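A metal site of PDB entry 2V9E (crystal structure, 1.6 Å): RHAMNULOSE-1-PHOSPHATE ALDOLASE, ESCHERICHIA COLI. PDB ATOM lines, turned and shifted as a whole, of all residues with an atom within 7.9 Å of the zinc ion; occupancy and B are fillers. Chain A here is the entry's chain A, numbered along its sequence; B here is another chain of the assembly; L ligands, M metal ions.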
ATOM      1  N   TRP A  25     -21.412  -9.590  -5.170  1.00  0.00           N
ATOM      2  CA  TRP A  25     -21.799  -8.309  -5.785  1.00  0.00           C
ATOM      3  C   TRP A  25     -23.209  -7.870  -5.440  1.00  0.00           C
ATOM      4  O   TRP A  25     -23.637  -6.781  -5.852  1.00  0.00           O
ATOM      5  CB  TRP A  25     -21.736  -8.420  -7.315  1.00  0.00           C
ATOM      6  CG  TRP A  25     -20.386  -8.715  -7.874  1.00  0.00           C
ATOM      7  CD1 TRP A  25     -19.158  -8.591  -7.259  1.00  0.00           C
ATOM      8  CD2 TRP A  25     -20.119  -9.124  -9.217  1.00  0.00           C
ATOM      9  NE1 TRP A  25     -18.152  -8.937  -8.125  1.00  0.00           N
ATOM     10  CE2 TRP A  25     -18.716  -9.256  -9.343  1.00  0.00           C
ATOM     11  CE3 TRP A  25     -20.935  -9.422 -10.320  1.00  0.00           C
ATOM     12  CZ2 TRP A  25     -18.104  -9.675 -10.537  1.00  0.00           C
ATOM     13  CZ3 TRP A  25     -20.331  -9.835 -11.511  1.00  0.00           C
ATOM     14  CH2 TRP A  25     -18.927  -9.950 -11.607  1.00  0.00           C
ATOM     15  N   ASP A  26     -23.971  -8.713  -4.741  1.00  0.00           N
ATOM     16  CA  ASP A  26     -25.407  -8.463  -4.626  1.00  0.00           C
ATOM     17  C   ASP A  26     -25.984  -8.865  -3.268  1.00  0.00           C
ATOM     18  O   ASP A  26     -26.903  -9.705  -3.178  1.00  0.00           O
ATOM     19  CB  ASP A  26     -26.165  -9.094  -5.805  1.00  0.00           C
ATOM     20  CG  ASP A  26     -25.756  -8.481  -7.127  1.00  0.00           C
ATOM     21  OD1 ASP A  26     -24.961  -9.099  -7.825  1.00  0.00           O
ATOM     22  OD2 ASP A  26     -26.210  -7.348  -7.439  1.00  0.00           O
ATOM     23  N   GLU A  27     -25.437  -8.237  -2.237  1.00  0.00           N
ATOM     24  CA  GLU A  27     -25.997  -8.289  -0.888  1.00  0.00           C
ATOM     25  C   GLU A  27     -27.470  -7.867  -0.868  1.00  0.00           C
ATOM     26  O   GLU A  27     -27.882  -7.002  -1.645  1.00  0.00           O
ATOM     27  CB  GLU A  27     -25.181  -7.391   0.051  1.00  0.00           C
ATOM     28  CG  GLU A  27     -25.375  -5.854  -0.151  1.00  0.00           C
ATOM     29  CD  GLU A  27     -24.581  -5.221  -1.310  1.00  0.00           C
ATOM     30  OE1 GLU A  27     -24.688  -3.965  -1.539  1.00  0.00           O
ATOM     31  OE2 GLU A  27     -23.849  -5.989  -1.992  1.00  0.00           O
ATOM     32  N   ASN A  29     -30.990  -6.817  -1.434  1.00  0.00           N
ATOM     33  CA  ASN A  29     -31.657  -6.621  -2.732  1.00  0.00           C
ATOM     34  C   ASN A  29     -30.827  -5.751  -3.676  1.00  0.00           C
ATOM     35  O   ASN A  29     -31.368  -5.186  -4.643  1.00  0.00           O
ATOM     36  CB  ASN A  29     -33.048  -5.998  -2.544  1.00  0.00           C
ATOM     37  CG  ASN A  29     -32.972  -4.622  -1.929  1.00  0.00           C
ATOM     38  OD1 ASN A  29     -32.233  -4.422  -0.963  1.00  0.00           O
ATOM     39  ND2 ASN A  29     -33.723  -3.664  -2.466  1.00  0.00           N
ATOM     40  N   GLY A  30     -29.522  -5.667  -3.413  1.00  0.00           N
ATOM     41  CA  GLY A  30     -28.606  -4.761  -4.116  1.00  0.00           C
ATOM     42  C   GLY A  30     -28.156  -5.230  -5.476  1.00  0.00           C
ATOM     43  O   GLY A  30     -27.007  -5.681  -5.653  1.00  0.00           O
ATOM     44  N   GLY A  31     -29.024  -5.041  -6.461  1.00  0.00           N
ATOM     45  CA  GLY A  31     -28.793  -5.505  -7.831  1.00  0.00           C
ATOM     46  C   GLY A  31     -30.111  -5.646  -8.558  1.00  0.00           C
ATOM     47  O   GLY A  31     -31.172  -5.832  -7.951  1.00  0.00           O
ATOM     48  N   ASN A  32     -30.057  -5.549  -9.875  1.00  0.00           N
ATOM     49  CA  ASN A  32     -31.241  -5.794 -10.694  1.00  0.00           C
ATOM     50  C   ASN A  32     -30.819  -6.119 -12.121  1.00  0.00           C
ATOM     51  O   ASN A  32     -29.758  -5.701 -12.584  1.00  0.00           O
ATOM     52  CB  ASN A  32     -32.268  -4.638 -10.650  1.00  0.00           C
ATOM     53  CG  ASN A  32     -31.657  -3.326 -10.224  1.00  0.00           C
ATOM     54  OD1 ASN A  32     -31.020  -2.645 -11.021  1.00  0.00           O
ATOM     55  ND2 ASN A  32     -31.865  -2.968  -8.958  1.00  0.00           N
ATOM     56  N   SER A 116     -37.213  -1.478  -8.521  1.00  0.00           N
ATOM     57  CA  SER A 116     -37.332  -0.034  -8.357  1.00  0.00           C
ATOM     58  C   SER A 116     -36.462   0.761  -9.330  1.00  0.00           C
ATOM     59  O   SER A 116     -36.648   1.982  -9.491  1.00  0.00           O
ATOM     60  CB  SER A 116     -36.965   0.376  -6.919  1.00  0.00           C
ATOM     61  OG  SER A 116     -35.638  -0.004  -6.626  1.00  0.00           O
ATOM     62  N   GLU A 117     -35.505   0.084  -9.985  1.00  0.00           N
ATOM     63  CA  GLU A 117     -34.623   0.742 -10.963  1.00  0.00           C
ATOM     64  C   GLU A 117     -35.107   0.524 -12.396  1.00  0.00           C
ATOM     65  O   GLU A 117     -34.344   0.689 -13.361  1.00  0.00           O
ATOM     66  CB  GLU A 117     -33.176   0.257 -10.816  1.00  0.00           C
ATOM     67  CG  GLU A 117     -32.539   0.640  -9.475  1.00  0.00           C
ATOM     68  CD  GLU A 117     -32.307   2.145  -9.301  1.00  0.00           C
ATOM     69  OE1 GLU A 117     -32.612   2.950 -10.201  1.00  0.00           O
ATOM     70  OE2 GLU A 117     -31.827   2.515  -8.222  1.00  0.00           O
ATOM     71  N   HIS A 141     -27.366  -4.466 -13.318  1.00  0.00           N
ATOM     72  CA  HIS A 141     -26.837  -3.593 -12.278  1.00  0.00           C
ATOM     73  C   HIS A 141     -26.409  -4.471 -11.124  1.00  0.00           C
ATOM     74  O   HIS A 141     -27.165  -5.334 -10.656  1.00  0.00           O
ATOM     75  CB  HIS A 141     -27.885  -2.592 -11.798  1.00  0.00           C
ATOM     76  CG  HIS A 141     -27.533  -1.896 -10.511  1.00  0.00           C
ATOM     77  ND1 HIS A 141     -26.386  -1.145 -10.353  1.00  0.00           N
ATOM     78  CD2 HIS A 141     -28.201  -1.830  -9.334  1.00  0.00           C
ATOM     79  CE1 HIS A 141     -26.360  -0.662  -9.114  1.00  0.00           C
ATOM     80  NE2 HIS A 141     -27.452  -1.049  -8.488  1.00  0.00           N
ATOM     81  N   CYS A 142     -25.231  -4.247 -10.589  1.00  0.00           N
ATOM     82  CA  CYS A 142     -24.903  -4.913  -9.313  1.00  0.00           C
ATOM     83  C   CYS A 142     -23.972  -3.965  -8.553  1.00  0.00           C
ATOM     84  O   CYS A 142     -23.611  -2.863  -9.018  1.00  0.00           O
ATOM     85  CB  CYS A 142     -24.183  -6.273  -9.538  1.00  0.00           C
ATOM     86  SG  CYS A 142     -22.599  -6.071 -10.551  1.00  0.00           S
ATOM     87  N   HIS A 143     -23.571  -4.455  -7.416  1.00  0.00           N
ATOM     88  CA  HIS A 143     -22.751  -3.717  -6.469  1.00  0.00           C
ATOM     89  C   HIS A 143     -21.351  -4.307  -6.468  1.00  0.00           C
ATOM     90  O   HIS A 143     -20.913  -4.936  -5.497  1.00  0.00           O
ATOM     91  CB  HIS A 143     -23.420  -3.716  -5.099  1.00  0.00           C
ATOM     92  CG  HIS A 143     -24.734  -2.993  -5.071  1.00  0.00           C
ATOM     93  ND1 HIS A 143     -25.451  -2.796  -3.906  1.00  0.00           N
ATOM     94  CD2 HIS A 143     -25.469  -2.415  -6.060  1.00  0.00           C
ATOM     95  CE1 HIS A 143     -26.550  -2.120  -4.173  1.00  0.00           C
ATOM     96  NE2 HIS A 143     -26.589  -1.865  -5.471  1.00  0.00           N
ATOM     97  N   ILE A 148     -16.758  -0.248  -6.824  1.00  0.00           N
ATOM     98  CA  ILE A 148     -17.278   0.675  -5.797  1.00  0.00           C
ATOM     99  C   ILE A 148     -16.128   1.304  -5.006  1.00  0.00           C
ATOM    100  O   ILE A 148     -16.055   2.527  -4.865  1.00  0.00           O
ATOM    101  CB  ILE A 148     -18.302  -0.011  -4.836  1.00  0.00           C
ATOM    102  CG1 ILE A 148     -19.578  -0.440  -5.572  1.00  0.00           C
ATOM    103  CG2 ILE A 148     -18.666   0.936  -3.675  1.00  0.00           C
ATOM    104  CD1 ILE A 148     -20.346  -1.468  -4.796  1.00  0.00           C
ATOM    105  N   PRO A 188     -30.780   7.130  -5.736  1.00  0.00           N
ATOM    106  CA  PRO A 188     -31.199   6.053  -6.619  1.00  0.00           C
ATOM    107  C   PRO A 188     -32.714   5.839  -6.663  1.00  0.00           C
ATOM    108  O   PRO A 188     -33.455   6.396  -5.848  1.00  0.00           O
ATOM    109  CB  PRO A 188     -30.483   4.821  -6.026  1.00  0.00           C
ATOM    110  CG  PRO A 188     -30.441   5.119  -4.582  1.00  0.00           C
ATOM    111  CD  PRO A 188     -30.236   6.620  -4.459  1.00  0.00           C
ATOM    112  N   GLY A 189     -33.167   5.061  -7.645  1.00  0.00           N
ATOM    113  CA  GLY A 189     -34.570   4.668  -7.777  1.00  0.00           C
ATOM    114  C   GLY A 189     -35.458   5.761  -8.328  1.00  0.00           C
ATOM    115  O   GLY A 189     -36.678   5.718  -8.170  1.00  0.00           O
ATOM    116  N   TRP A 209     -22.074   4.244 -10.948  1.00  0.00           N
ATOM    117  CA  TRP A 209     -22.784   5.020  -9.935  1.00  0.00           C
ATOM    118  C   TRP A 209     -21.852   5.110  -8.734  1.00  0.00           C
ATOM    119  O   TRP A 209     -21.697   4.120  -8.004  1.00  0.00           O
ATOM    120  CB  TRP A 209     -24.077   4.288  -9.559  1.00  0.00           C
ATOM    121  CG  TRP A 209     -25.177   4.391 -10.567  1.00  0.00           C
ATOM    122  CD1 TRP A 209     -25.112   4.896 -11.846  1.00  0.00           C
ATOM    123  CD2 TRP A 209     -26.530   3.972 -10.367  1.00  0.00           C
ATOM    124  NE1 TRP A 209     -26.355   4.818 -12.450  1.00  0.00           N
ATOM    125  CE2 TRP A 209     -27.249   4.272 -11.566  1.00  0.00           C
ATOM    126  CE3 TRP A 209     -27.220   3.386  -9.297  1.00  0.00           C
ATOM    127  CZ2 TRP A 209     -28.615   3.982 -11.705  1.00  0.00           C
ATOM    128  CZ3 TRP A 209     -28.589   3.113  -9.439  1.00  0.00           C
ATOM    129  CH2 TRP A 209     -29.275   3.426 -10.639  1.00  0.00           C
ATOM    130  N   HIS A 212     -21.888   3.293  -5.092  1.00  0.00           N
ATOM    131  CA  HIS A 212     -23.089   2.481  -5.254  1.00  0.00           C
ATOM    132  C   HIS A 212     -22.858   1.225  -6.089  1.00  0.00           C
ATOM    133  O   HIS A 212     -23.004   0.108  -5.608  1.00  0.00           O
ATOM    134  CB  HIS A 212     -24.261   3.337  -5.784  1.00  0.00           C
ATOM    135  CG  HIS A 212     -25.557   2.598  -5.897  1.00  0.00           C
ATOM    136  ND1 HIS A 212     -26.783   3.233  -5.891  1.00  0.00           N
ATOM    137  CD2 HIS A 212     -25.829   1.269  -5.989  1.00  0.00           C
ATOM    138  CE1 HIS A 212     -27.751   2.331  -6.005  1.00  0.00           C
ATOM    139  NE2 HIS A 212     -27.189   1.137  -6.062  1.00  0.00           N
ATOM    140  N   GLY A 213     -22.506   1.378  -7.365  1.00  0.00           N
ATOM    141  CA  GLY A 213     -22.310   0.196  -8.183  1.00  0.00           C
ATOM    142  C   GLY A 213     -22.162   0.507  -9.649  1.00  0.00           C
ATOM    143  O   GLY A 213     -21.707   1.588 -10.020  1.00  0.00           O
ATOM    144  N   VAL A 214     -22.538  -0.464 -10.474  1.00  0.00           N
ATOM    145  CA  VAL A 214     -22.261  -0.390 -11.912  1.00  0.00           C
ATOM    146  C   VAL A 214     -23.479  -0.861 -12.710  1.00  0.00           C
ATOM    147  O   VAL A 214     -24.252  -1.700 -12.229  1.00  0.00           O
ATOM    148  CB  VAL A 214     -20.970  -1.196 -12.280  1.00  0.00           C
ATOM    149  CG1 VAL A 214     -21.179  -2.715 -12.089  1.00  0.00           C
ATOM    150  CG2 VAL A 214     -20.470  -0.875 -13.690  1.00  0.00           C
ATOM    151  N   PHE A 215     -23.662  -0.291 -13.901  1.00  0.00           N
ATOM    152  CA  PHE A 215     -24.617  -0.772 -14.888  1.00  0.00           C
ATOM    153  C   PHE A 215     -23.838  -1.216 -16.127  1.00  0.00           C
ATOM    154  O   PHE A 215     -22.905  -0.538 -16.565  1.00  0.00           O
ATOM    155  CB  PHE A 215     -25.594   0.341 -15.303  1.00  0.00           C
ATOM    156  CG  PHE A 215     -26.795   0.427 -14.442  1.00  0.00           C
ATOM    157  CD1 PHE A 215     -26.694   0.898 -13.135  1.00  0.00           C
ATOM    158  CD2 PHE A 215     -28.040  -0.009 -14.911  1.00  0.00           C
ATOM    159  CE1 PHE A 215     -27.838   0.964 -12.316  1.00  0.00           C
ATOM    160  CE2 PHE A 215     -29.180   0.069 -14.099  1.00  0.00           C
ATOM    161  CZ  PHE A 215     -29.080   0.543 -12.801  1.00  0.00           C
ATOM    162  N   THR B 170     -24.265   3.117  -0.839  1.00  0.00           N
ATOM    163  CA  THR B 170     -25.420   4.031  -0.872  1.00  0.00           C
ATOM    164  C   THR B 170     -26.641   3.536  -0.100  1.00  0.00           C
ATOM    165  O   THR B 170     -27.279   4.316   0.602  1.00  0.00           O
ATOM    166  CB  THR B 170     -25.768   4.399  -2.326  1.00  0.00           C
ATOM    167  OG1 THR B 170     -24.757   5.259  -2.845  1.00  0.00           O
ATOM    168  CG2 THR B 170     -27.138   5.118  -2.411  1.00  0.00           C
ATOM    169  N   GLU B 171     -26.959   2.247  -0.210  1.00  0.00           N
ATOM    170  CA  GLU B 171     -28.193   1.758   0.390  1.00  0.00           C
ATOM    171  C   GLU B 171     -28.133   1.606   1.916  1.00  0.00           C
ATOM    172  O   GLU B 171     -29.159   1.323   2.541  1.00  0.00           O
ATOM    173  CB  GLU B 171     -28.582   0.438  -0.260  1.00  0.00           C
ATOM    174  CG  GLU B 171     -27.723  -0.720   0.181  1.00  0.00           C
ATOM    175  CD  GLU B 171     -26.453  -0.987  -0.638  1.00  0.00           C
ATOM    176  OE1 GLU B 171     -25.895  -2.065  -0.346  1.00  0.00           O
ATOM    177  OE2 GLU B 171     -26.010  -0.171  -1.516  1.00  0.00           O
HETATM  178  C1  LIG L   1     -30.403  -1.325  -5.610  1.00  0.00           C
HETATM  179  O1  LIG L   1     -29.929  -1.227  -6.745  1.00  0.00           O
HETATM  180  O2  LIG L   1     -29.671  -1.180  -4.611  1.00  0.00           O
HETATM  181  C2  LIG L   1     -31.851  -1.647  -5.448  1.00  0.00           C
HETATM  182 ZN    ZN M   1     -27.978  -0.708  -6.492  1.00  0.00          ZN
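A ring nitrogen (ND1) of His 143 is in hydrogen-bond range of the side-chain carboxylate (OE1) of Glu 27 (2.7 Å).
The backbone carbonyl oxygen (O) of Trp 25 sits at hydrogen-bond distance from the backbone NH (N) of His 143, at 2.8 Å.
N of His 141 is in hydrogen-bond range of O of Asn 32 (2.8 Å).
The backbone carbonyl oxygen (O) of Val 214 is in hydrogen-bond range of a ring nitrogen (ND1) of His 141 (2.9 Å).
Three residues have an atom within 4 Å of the zinc ion: His 141, His 143 and His 212.
The nearest printed residue that does not touch the zinc ion is Gly 31 (4.5 Å).
The zinc ion is bound by O1 of the ligand.
NE2 of His 212 binds the zinc ion (2.1 Å).
The zinc ion is bound by NE2 of His 143 (2.1 Å).
A ring nitrogen (NE2) of His 141 binds the zinc ion, at 2.1 Å.
O2 of the ligand binds the zinc ion, at 2.6 Å.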
